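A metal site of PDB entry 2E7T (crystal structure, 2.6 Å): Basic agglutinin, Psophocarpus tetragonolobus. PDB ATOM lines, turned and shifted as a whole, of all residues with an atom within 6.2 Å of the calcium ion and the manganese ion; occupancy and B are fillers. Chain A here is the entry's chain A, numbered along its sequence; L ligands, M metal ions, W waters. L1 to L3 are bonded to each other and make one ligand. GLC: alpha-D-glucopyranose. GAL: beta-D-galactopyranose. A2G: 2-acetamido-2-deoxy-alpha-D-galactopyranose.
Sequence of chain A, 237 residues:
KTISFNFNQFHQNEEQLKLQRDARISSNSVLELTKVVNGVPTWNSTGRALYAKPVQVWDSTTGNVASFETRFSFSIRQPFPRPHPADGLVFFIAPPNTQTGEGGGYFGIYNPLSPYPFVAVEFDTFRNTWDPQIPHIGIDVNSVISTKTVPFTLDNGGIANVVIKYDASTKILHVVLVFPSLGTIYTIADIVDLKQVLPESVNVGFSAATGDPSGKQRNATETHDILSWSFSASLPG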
ATOM      1  N   ASP A  87      18.593  -0.772  28.373  1.00  0.00           N
ATOM      2  CA  ASP A  87      17.997  -0.847  27.046  1.00  0.00           C
ATOM      3  C   ASP A  87      16.525  -1.221  27.119  1.00  0.00           C
ATOM      4  O   ASP A  87      15.731  -0.828  26.249  1.00  0.00           O
ATOM      5  CB  ASP A  87      18.726  -1.876  26.171  1.00  0.00           C
ATOM      6  CG  ASP A  87      19.943  -1.285  25.459  1.00  0.00           C
ATOM      7  OD1 ASP A  87      21.072  -1.329  26.024  1.00  0.00           O
ATOM      8  OD2 ASP A  87      19.776  -0.772  24.324  1.00  0.00           O
ATOM      9  N   GLY A 104      22.641  -5.342  25.089  1.00  0.00           N
ATOM     10  CA  GLY A 104      22.239  -4.124  24.431  1.00  0.00           C
ATOM     11  C   GLY A 104      20.830  -4.171  23.865  1.00  0.00           C
ATOM     12  O   GLY A 104      19.904  -4.635  24.533  1.00  0.00           O
ATOM     13  N   GLY A 105      20.672  -3.684  22.641  1.00  0.00           N
ATOM     14  CA  GLY A 105      19.369  -3.653  21.998  1.00  0.00           C
ATOM     15  C   GLY A 105      18.831  -5.018  21.644  1.00  0.00           C
ATOM     16  O   GLY A 105      17.721  -5.114  21.094  1.00  0.00           O
ATOM     17  N   PHE A 107      18.424  -7.269  23.977  1.00  0.00           N
ATOM     18  CA  PHE A 107      17.799  -7.679  25.246  1.00  0.00           C
ATOM     19  C   PHE A 107      18.288  -8.992  25.849  1.00  0.00           C
ATOM     20  O   PHE A 107      17.802  -9.402  26.882  1.00  0.00           O
ATOM     21  CB  PHE A 107      16.276  -7.755  25.082  1.00  0.00           C
ATOM     22  CG  PHE A 107      15.647  -6.509  24.502  1.00  0.00           C
ATOM     23  CD1 PHE A 107      15.675  -5.309  25.201  1.00  0.00           C
ATOM     24  CD2 PHE A 107      15.012  -6.545  23.267  1.00  0.00           C
ATOM     25  CE1 PHE A 107      15.056  -4.164  24.694  1.00  0.00           C
ATOM     26  CE2 PHE A 107      14.398  -5.411  22.754  1.00  0.00           C
ATOM     27  CZ  PHE A 107      14.412  -4.212  23.468  1.00  0.00           C
ATOM     28  N   GLU A 122       8.333  -6.579  24.156  1.00  0.00           N
ATOM     29  CA  GLU A 122       9.360  -5.710  24.673  1.00  0.00           C
ATOM     30  C   GLU A 122       8.881  -4.370  25.226  1.00  0.00           C
ATOM     31  O   GLU A 122       7.861  -3.820  24.811  1.00  0.00           O
ATOM     32  CB  GLU A 122      10.390  -5.438  23.595  1.00  0.00           C
ATOM     33  CG  GLU A 122       9.816  -4.645  22.438  1.00  0.00           C
ATOM     34  CD  GLU A 122      10.874  -4.129  21.469  1.00  0.00           C
ATOM     35  OE1 GLU A 122      11.608  -4.954  20.890  1.00  0.00           O
ATOM     36  OE2 GLU A 122      10.957  -2.883  21.287  1.00  0.00           O
ATOM     37  N   ASP A 124      10.890  -1.356  25.369  1.00  0.00           N
ATOM     38  CA  ASP A 124      12.098  -0.757  24.854  1.00  0.00           C
ATOM     39  C   ASP A 124      12.305   0.653  25.296  1.00  0.00           C
ATOM     40  O   ASP A 124      11.429   1.495  25.070  1.00  0.00           O
ATOM     41  CB  ASP A 124      12.035  -0.815  23.332  1.00  0.00           C
ATOM     42  CG  ASP A 124      13.404  -0.775  22.691  1.00  0.00           C
ATOM     43  OD1 ASP A 124      14.324  -0.180  23.287  1.00  0.00           O
ATOM     44  OD2 ASP A 124      13.557  -1.345  21.604  1.00  0.00           O
ATOM     45  N   THR A 125      13.475   0.939  25.857  1.00  0.00           N
ATOM     46  CA  THR A 125      13.757   2.287  26.347  1.00  0.00           C
ATOM     47  C   THR A 125      14.861   3.059  25.617  1.00  0.00           C
ATOM     48  O   THR A 125      15.032   4.259  25.842  1.00  0.00           O
ATOM     49  CB  THR A 125      14.081   2.227  27.836  1.00  0.00           C
ATOM     50  OG1 THR A 125      15.194   1.359  28.052  1.00  0.00           O
ATOM     51  CG2 THR A 125      12.870   1.676  28.614  1.00  0.00           C
ATOM     52  N   PHE A 126      15.621   2.381  24.752  1.00  0.00           N
ATOM     53  CA  PHE A 126      16.706   2.991  24.013  1.00  0.00           C
ATOM     54  C   PHE A 126      16.384   2.870  22.546  1.00  0.00           C
ATOM     55  O   PHE A 126      15.921   1.822  22.098  1.00  0.00           O
ATOM     56  CB  PHE A 126      18.025   2.270  24.284  1.00  0.00           C
ATOM     57  CG  PHE A 126      19.148   2.769  23.438  1.00  0.00           C
ATOM     58  CD1 PHE A 126      19.833   3.930  23.776  1.00  0.00           C
ATOM     59  CD2 PHE A 126      19.522   2.077  22.283  1.00  0.00           C
ATOM     60  CE1 PHE A 126      20.885   4.402  22.986  1.00  0.00           C
ATOM     61  CE2 PHE A 126      20.567   2.531  21.486  1.00  0.00           C
ATOM     62  CZ  PHE A 126      21.256   3.700  21.827  1.00  0.00           C
ATOM     63  N   ARG A 127      16.618   3.936  21.781  1.00  0.00           N
ATOM     64  CA  ARG A 127      16.310   3.897  20.352  1.00  0.00           C
ATOM     65  C   ARG A 127      17.443   3.461  19.443  1.00  0.00           C
ATOM     66  O   ARG A 127      18.340   4.251  19.181  1.00  0.00           O
ATOM     67  CB  ARG A 127      15.788   5.254  19.877  1.00  0.00           C
ATOM     68  CG  ARG A 127      15.437   5.249  18.410  1.00  0.00           C
ATOM     69  CD  ARG A 127      14.746   6.538  17.993  1.00  0.00           C
ATOM     70  NE  ARG A 127      14.115   6.380  16.681  1.00  0.00           N
ATOM     71  CZ  ARG A 127      13.323   7.285  16.117  1.00  0.00           C
ATOM     72  NH1 ARG A 127      13.063   8.419  16.759  1.00  0.00           N
ATOM     73  NH2 ARG A 127      12.762   7.043  14.949  1.00  0.00           N
ATOM     74  N   ASN A 128      17.395   2.232  18.960  1.00  0.00           N
ATOM     75  CA  ASN A 128      18.414   1.754  18.043  1.00  0.00           C
ATOM     76  C   ASN A 128      18.057   2.188  16.634  1.00  0.00           C
ATOM     77  O   ASN A 128      17.002   2.779  16.417  1.00  0.00           O
ATOM     78  CB  ASN A 128      18.529   0.226  18.091  1.00  0.00           C
ATOM     79  CG  ASN A 128      18.996  -0.272  19.429  1.00  0.00           C
ATOM     80  OD1 ASN A 128      18.218  -0.353  20.370  1.00  0.00           O
ATOM     81  ND2 ASN A 128      20.262  -0.594  19.529  1.00  0.00           N
ATOM     82  N   TRP A 130      16.990   0.578  14.261  1.00  0.00           N
ATOM     83  CA  TRP A 130      15.757  -0.075  13.822  1.00  0.00           C
ATOM     84  C   TRP A 130      14.502   0.275  14.609  1.00  0.00           C
ATOM     85  O   TRP A 130      13.435  -0.266  14.327  1.00  0.00           O
ATOM     86  CB  TRP A 130      15.965  -1.581  13.862  1.00  0.00           C
ATOM     87  CG  TRP A 130      16.211  -2.096  15.243  1.00  0.00           C
ATOM     88  CD1 TRP A 130      15.287  -2.257  16.249  1.00  0.00           C
ATOM     89  CD2 TRP A 130      17.474  -2.501  15.794  1.00  0.00           C
ATOM     90  NE1 TRP A 130      15.900  -2.736  17.382  1.00  0.00           N
ATOM     91  CE2 TRP A 130      17.235  -2.891  17.133  1.00  0.00           C
ATOM     92  CE3 TRP A 130      18.786  -2.581  15.286  1.00  0.00           C
ATOM     93  CZ2 TRP A 130      18.253  -3.364  17.968  1.00  0.00           C
ATOM     94  CZ3 TRP A 130      19.799  -3.042  16.129  1.00  0.00           C
ATOM     95  CH2 TRP A 130      19.530  -3.423  17.447  1.00  0.00           C
ATOM     96  N   ASP A 131      14.628   1.196  15.563  1.00  0.00           N
ATOM     97  CA  ASP A 131      13.526   1.613  16.428  1.00  0.00           C
ATOM     98  C   ASP A 131      12.810   2.904  16.150  1.00  0.00           C
ATOM     99  O   ASP A 131      13.374   3.839  15.605  1.00  0.00           O
ATOM    100  CB  ASP A 131      14.000   1.794  17.876  1.00  0.00           C
ATOM    101  CG  ASP A 131      14.221   0.502  18.593  1.00  0.00           C
ATOM    102  OD1 ASP A 131      13.454  -0.466  18.349  1.00  0.00           O
ATOM    103  OD2 ASP A 131      15.159   0.499  19.432  1.00  0.00           O
ATOM    104  N   PRO A 132      11.534   2.984  16.564  1.00  0.00           N
ATOM    105  CA  PRO A 132      10.729   4.183  16.408  1.00  0.00           C
ATOM    106  C   PRO A 132      10.984   4.902  17.744  1.00  0.00           C
ATOM    107  O   PRO A 132      11.715   4.381  18.567  1.00  0.00           O
ATOM    108  CB  PRO A 132       9.307   3.633  16.289  1.00  0.00           C
ATOM    109  CG  PRO A 132       9.345   2.477  17.175  1.00  0.00           C
ATOM    110  CD  PRO A 132      10.668   1.817  16.815  1.00  0.00           C
ATOM    111  N   ILE A 134      11.179   6.108  21.484  1.00  0.00           N
ATOM    112  CA  ILE A 134      11.060   5.330  22.718  1.00  0.00           C
ATOM    113  C   ILE A 134      10.546   6.210  23.866  1.00  0.00           C
ATOM    114  O   ILE A 134      10.602   7.429  23.810  1.00  0.00           O
ATOM    115  CB  ILE A 134      12.415   4.677  23.131  1.00  0.00           C
ATOM    116  CG1 ILE A 134      13.564   5.683  23.136  1.00  0.00           C
ATOM    117  CG2 ILE A 134      12.723   3.555  22.171  1.00  0.00           C
ATOM    118  CD1 ILE A 134      13.595   6.628  24.335  1.00  0.00           C
ATOM    119  N   HIS A 136       8.640   2.352  24.009  1.00  0.00           N
ATOM    120  CA  HIS A 136       7.521   1.787  23.283  1.00  0.00           C
ATOM    121  C   HIS A 136       7.344   0.312  23.623  1.00  0.00           C
ATOM    122  O   HIS A 136       8.264  -0.347  24.097  1.00  0.00           O
ATOM    123  CB  HIS A 136       7.677   1.950  21.758  1.00  0.00           C
ATOM    124  CG  HIS A 136       8.945   1.372  21.188  1.00  0.00           C
ATOM    125  ND1 HIS A 136      10.059   2.147  20.941  1.00  0.00           N
ATOM    126  CD2 HIS A 136       9.250   0.119  20.775  1.00  0.00           C
ATOM    127  CE1 HIS A 136      11.002   1.383  20.394  1.00  0.00           C
ATOM    128  NE2 HIS A 136      10.539   0.159  20.279  1.00  0.00           N
ATOM    129  N   GLY A 138       6.496  -3.342  22.123  1.00  0.00           N
ATOM    130  CA  GLY A 138       6.652  -3.913  20.798  1.00  0.00           C
ATOM    131  C   GLY A 138       6.429  -5.406  20.850  1.00  0.00           C
ATOM    132  O   GLY A 138       6.686  -6.055  21.883  1.00  0.00           O
ATOM    133  N   ASP A 140       7.624  -8.806  19.185  1.00  0.00           N
ATOM    134  CA  ASP A 140       8.714  -9.342  18.402  1.00  0.00           C
ATOM    135  C   ASP A 140       8.571 -10.815  18.082  1.00  0.00           C
ATOM    136  O   ASP A 140       8.250 -11.613  18.960  1.00  0.00           O
ATOM    137  CB  ASP A 140      10.039  -9.120  19.137  1.00  0.00           C
ATOM    138  CG  ASP A 140      10.270  -7.658  19.481  1.00  0.00           C
ATOM    139  OD1 ASP A 140       9.678  -6.763  18.820  1.00  0.00           O
ATOM    140  OD2 ASP A 140      11.065  -7.397  20.414  1.00  0.00           O
ATOM    141  N   VAL A 144      14.171  -8.427  16.906  1.00  0.00           N
ATOM    142  CA  VAL A 144      13.875  -7.255  17.722  1.00  0.00           C
ATOM    143  C   VAL A 144      13.322  -6.149  16.865  1.00  0.00           C
ATOM    144  O   VAL A 144      13.164  -5.032  17.323  1.00  0.00           O
ATOM    145  CB  VAL A 144      15.104  -6.742  18.466  1.00  0.00           C
ATOM    146  CG1 VAL A 144      15.574  -7.811  19.465  1.00  0.00           C
ATOM    147  CG2 VAL A 144      16.195  -6.426  17.474  1.00  0.00           C
ATOM    148  N   SER A 146      10.316  -5.175  15.762  1.00  0.00           N
ATOM    149  CA  SER A 146       8.898  -5.402  16.049  1.00  0.00           C
ATOM    150  C   SER A 146       7.963  -5.367  14.859  1.00  0.00           C
ATOM    151  O   SER A 146       8.150  -4.593  13.919  1.00  0.00           O
ATOM    152  CB  SER A 146       8.416  -4.356  17.062  1.00  0.00           C
ATOM    153  OG  SER A 146       9.286  -4.308  18.165  1.00  0.00           O
ATOM    154  N   THR A 149       4.145  -1.761  17.128  1.00  0.00           N
ATOM    155  CA  THR A 149       4.713  -0.952  18.193  1.00  0.00           C
ATOM    156  C   THR A 149       3.766   0.158  18.653  1.00  0.00           C
ATOM    157  O   THR A 149       2.975   0.676  17.872  1.00  0.00           O
ATOM    158  CB  THR A 149       6.038  -0.316  17.694  1.00  0.00           C
ATOM    159  OG1 THR A 149       7.080  -1.301  17.670  1.00  0.00           O
ATOM    160  CG2 THR A 149       6.458   0.830  18.586  1.00  0.00           C
HETATM  161  C1  GLC L   1      31.001   4.858  16.083  1.00  0.00           C
HETATM  162  C2  GLC L   1      31.457   4.740  17.520  1.00  0.00           C
HETATM  163  C3  GLC L   1      30.594   3.757  18.270  1.00  0.00           C
HETATM  164  C4  GLC L   1      29.103   4.060  18.131  1.00  0.00           C
HETATM  165  C5  GLC L   1      28.735   4.293  16.630  1.00  0.00           C
HETATM  166  C6  GLC L   1      27.308   4.815  16.396  1.00  0.00           C
HETATM  167  O1  GLC L   1      31.118   3.636  15.466  1.00  0.00           O
HETATM  168  O2  GLC L   1      32.805   4.302  17.565  1.00  0.00           O
HETATM  169  O3  GLC L   1      30.944   3.814  19.635  1.00  0.00           O
HETATM  170  O4  GLC L   1      28.366   2.956  18.703  1.00  0.00           O
HETATM  171  O5  GLC L   1      29.624   5.261  16.041  1.00  0.00           O
HETATM  172  O6  GLC L   1      27.120   5.286  15.067  1.00  0.00           O
HETATM  173  C1  GAL L   2      26.990   3.029  18.710  1.00  0.00           C
HETATM  174  C2  GAL L   2      26.382   2.060  19.712  1.00  0.00           C
HETATM  175  C3  GAL L   2      24.875   2.236  19.652  1.00  0.00           C
HETATM  176  C4  GAL L   2      24.501   3.675  19.869  1.00  0.00           C
HETATM  177  C5  GAL L   2      25.211   4.574  18.878  1.00  0.00           C
HETATM  178  C6  GAL L   2      24.938   6.038  19.132  1.00  0.00           C
HETATM  179  O2  GAL L   2      26.743   0.736  19.360  1.00  0.00           O
HETATM  180  O3  GAL L   2      24.152   1.431  20.591  1.00  0.00           O
HETATM  181  O4  GAL L   2      24.885   4.041  21.174  1.00  0.00           O
HETATM  182  O5  GAL L   2      26.622   4.360  19.020  1.00  0.00           O
HETATM  183  O6  GAL L   2      26.059   6.838  18.813  1.00  0.00           O
HETATM  184  O5  A2G L   3      24.979   1.157  22.742  1.00  0.00           O
HETATM  185  C1  A2G L   3      24.762   0.542  21.484  1.00  0.00           C
HETATM  186  C2  A2G L   3      23.817  -0.666  21.658  1.00  0.00           C
HETATM  187  N2  A2G L   3      23.574  -1.296  20.378  1.00  0.00           N
HETATM  188  C3  A2G L   3      22.504  -0.180  22.276  1.00  0.00           C
HETATM  189  O3  A2G L   3      21.594  -1.222  22.491  1.00  0.00           O
HETATM  190  C4  A2G L   3      22.785   0.531  23.575  1.00  0.00           C
HETATM  191  O4  A2G L   3      23.285  -0.388  24.513  1.00  0.00           O
HETATM  192  C5  A2G L   3      23.785   1.649  23.394  1.00  0.00           C
HETATM  193  C6  A2G L   3      24.212   2.165  24.741  1.00  0.00           C
HETATM  194  O6  A2G L   3      24.628   3.504  24.673  1.00  0.00           O
HETATM  195  C7  A2G L   3      23.583  -2.610  20.256  1.00  0.00           C
HETATM  196  O7  A2G L   3      23.836  -3.355  21.158  1.00  0.00           O
HETATM  197  C8  A2G L   3      23.239  -3.148  18.905  1.00  0.00           C
HETATM  198 CA    CA M   1      16.132  -0.733  21.580  1.00  0.00          CA
HETATM  199 MN    MN M   2      12.203  -1.762  19.808  1.00  0.00          MN
HETATM  200  O   HOH W   1      10.884  -2.122  17.888  1.00  0.00           O
HETATM  201  O   HOH W   2      15.930  -3.196  20.412  1.00  0.00           O
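An oxygen (O3) of A2G L3 sits at hydrogen-bond distance from the side-chain amide nitrogen (ND2) of Asn 128.
The backbone NH of Gly 105 is in hydrogen-bond range of an oxygen (O3) of A2G L3, 2.6 Å away.
The side-chain carboxylate of Asp 87 is in hydrogen-bond range of an oxygen (O3) of A2G L3.
The side-chain carboxylate of Glu 122 sits close to the side-chain carboxylate of Asp 140, at 2.5 Å.
O of Asp 131 lies within hydrogen-bond range of NE of Arg 127 (2.9 Å).
OD1 of Asp 131 sits close to NE1 of Trp 130, 3.5 Å away.
O of Gly 138 is in hydrogen-bond range of N of Glu 122, 2.9 Å away.
Within 4 Å of the calcium ion: Asp 124, Phe 126, Asn 128 and Asp 131.
Within 4 Å of the manganese ion: Glu 122, Asp 124, Asp 131 and His 136.
The nearest printed residue that does not touch the manganese ion is Ser 146 (4.2 Å).
The calcium ion is bound by the side-chain amide oxygen (OD1) of Asn 128 (2.4 Å), the side-chain carboxylate (OD1) of Asp 124 (2.5 Å), the backbone carbonyl oxygen (O) of Phe 126 (2.6 Å), the side-chain carboxylate (OD2) of Asp 124 (2.6 Å), the side-chain carboxylate (OD2) of Asp 131 (2.7 Å) and water W2 (2.7 Å).
The calcium ion has six donor atoms within binding distance.
The manganese ion is bound by the side-chain carboxylate of Glu 122 (2.2 Å), the side-chain carboxylate of Asp 124 (2.3 Å), the side-chain carboxylate of Asp 131 (2.3 Å), water W1 (2.4 Å) and a ring nitrogen (NE2) of His 136 (2.6 Å).
The manganese ion has five donor atoms within binding distance.
Water W2 bridges O of Gly 105 (2.7 Å) and NE1 of Trp 130 (3.1 Å).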
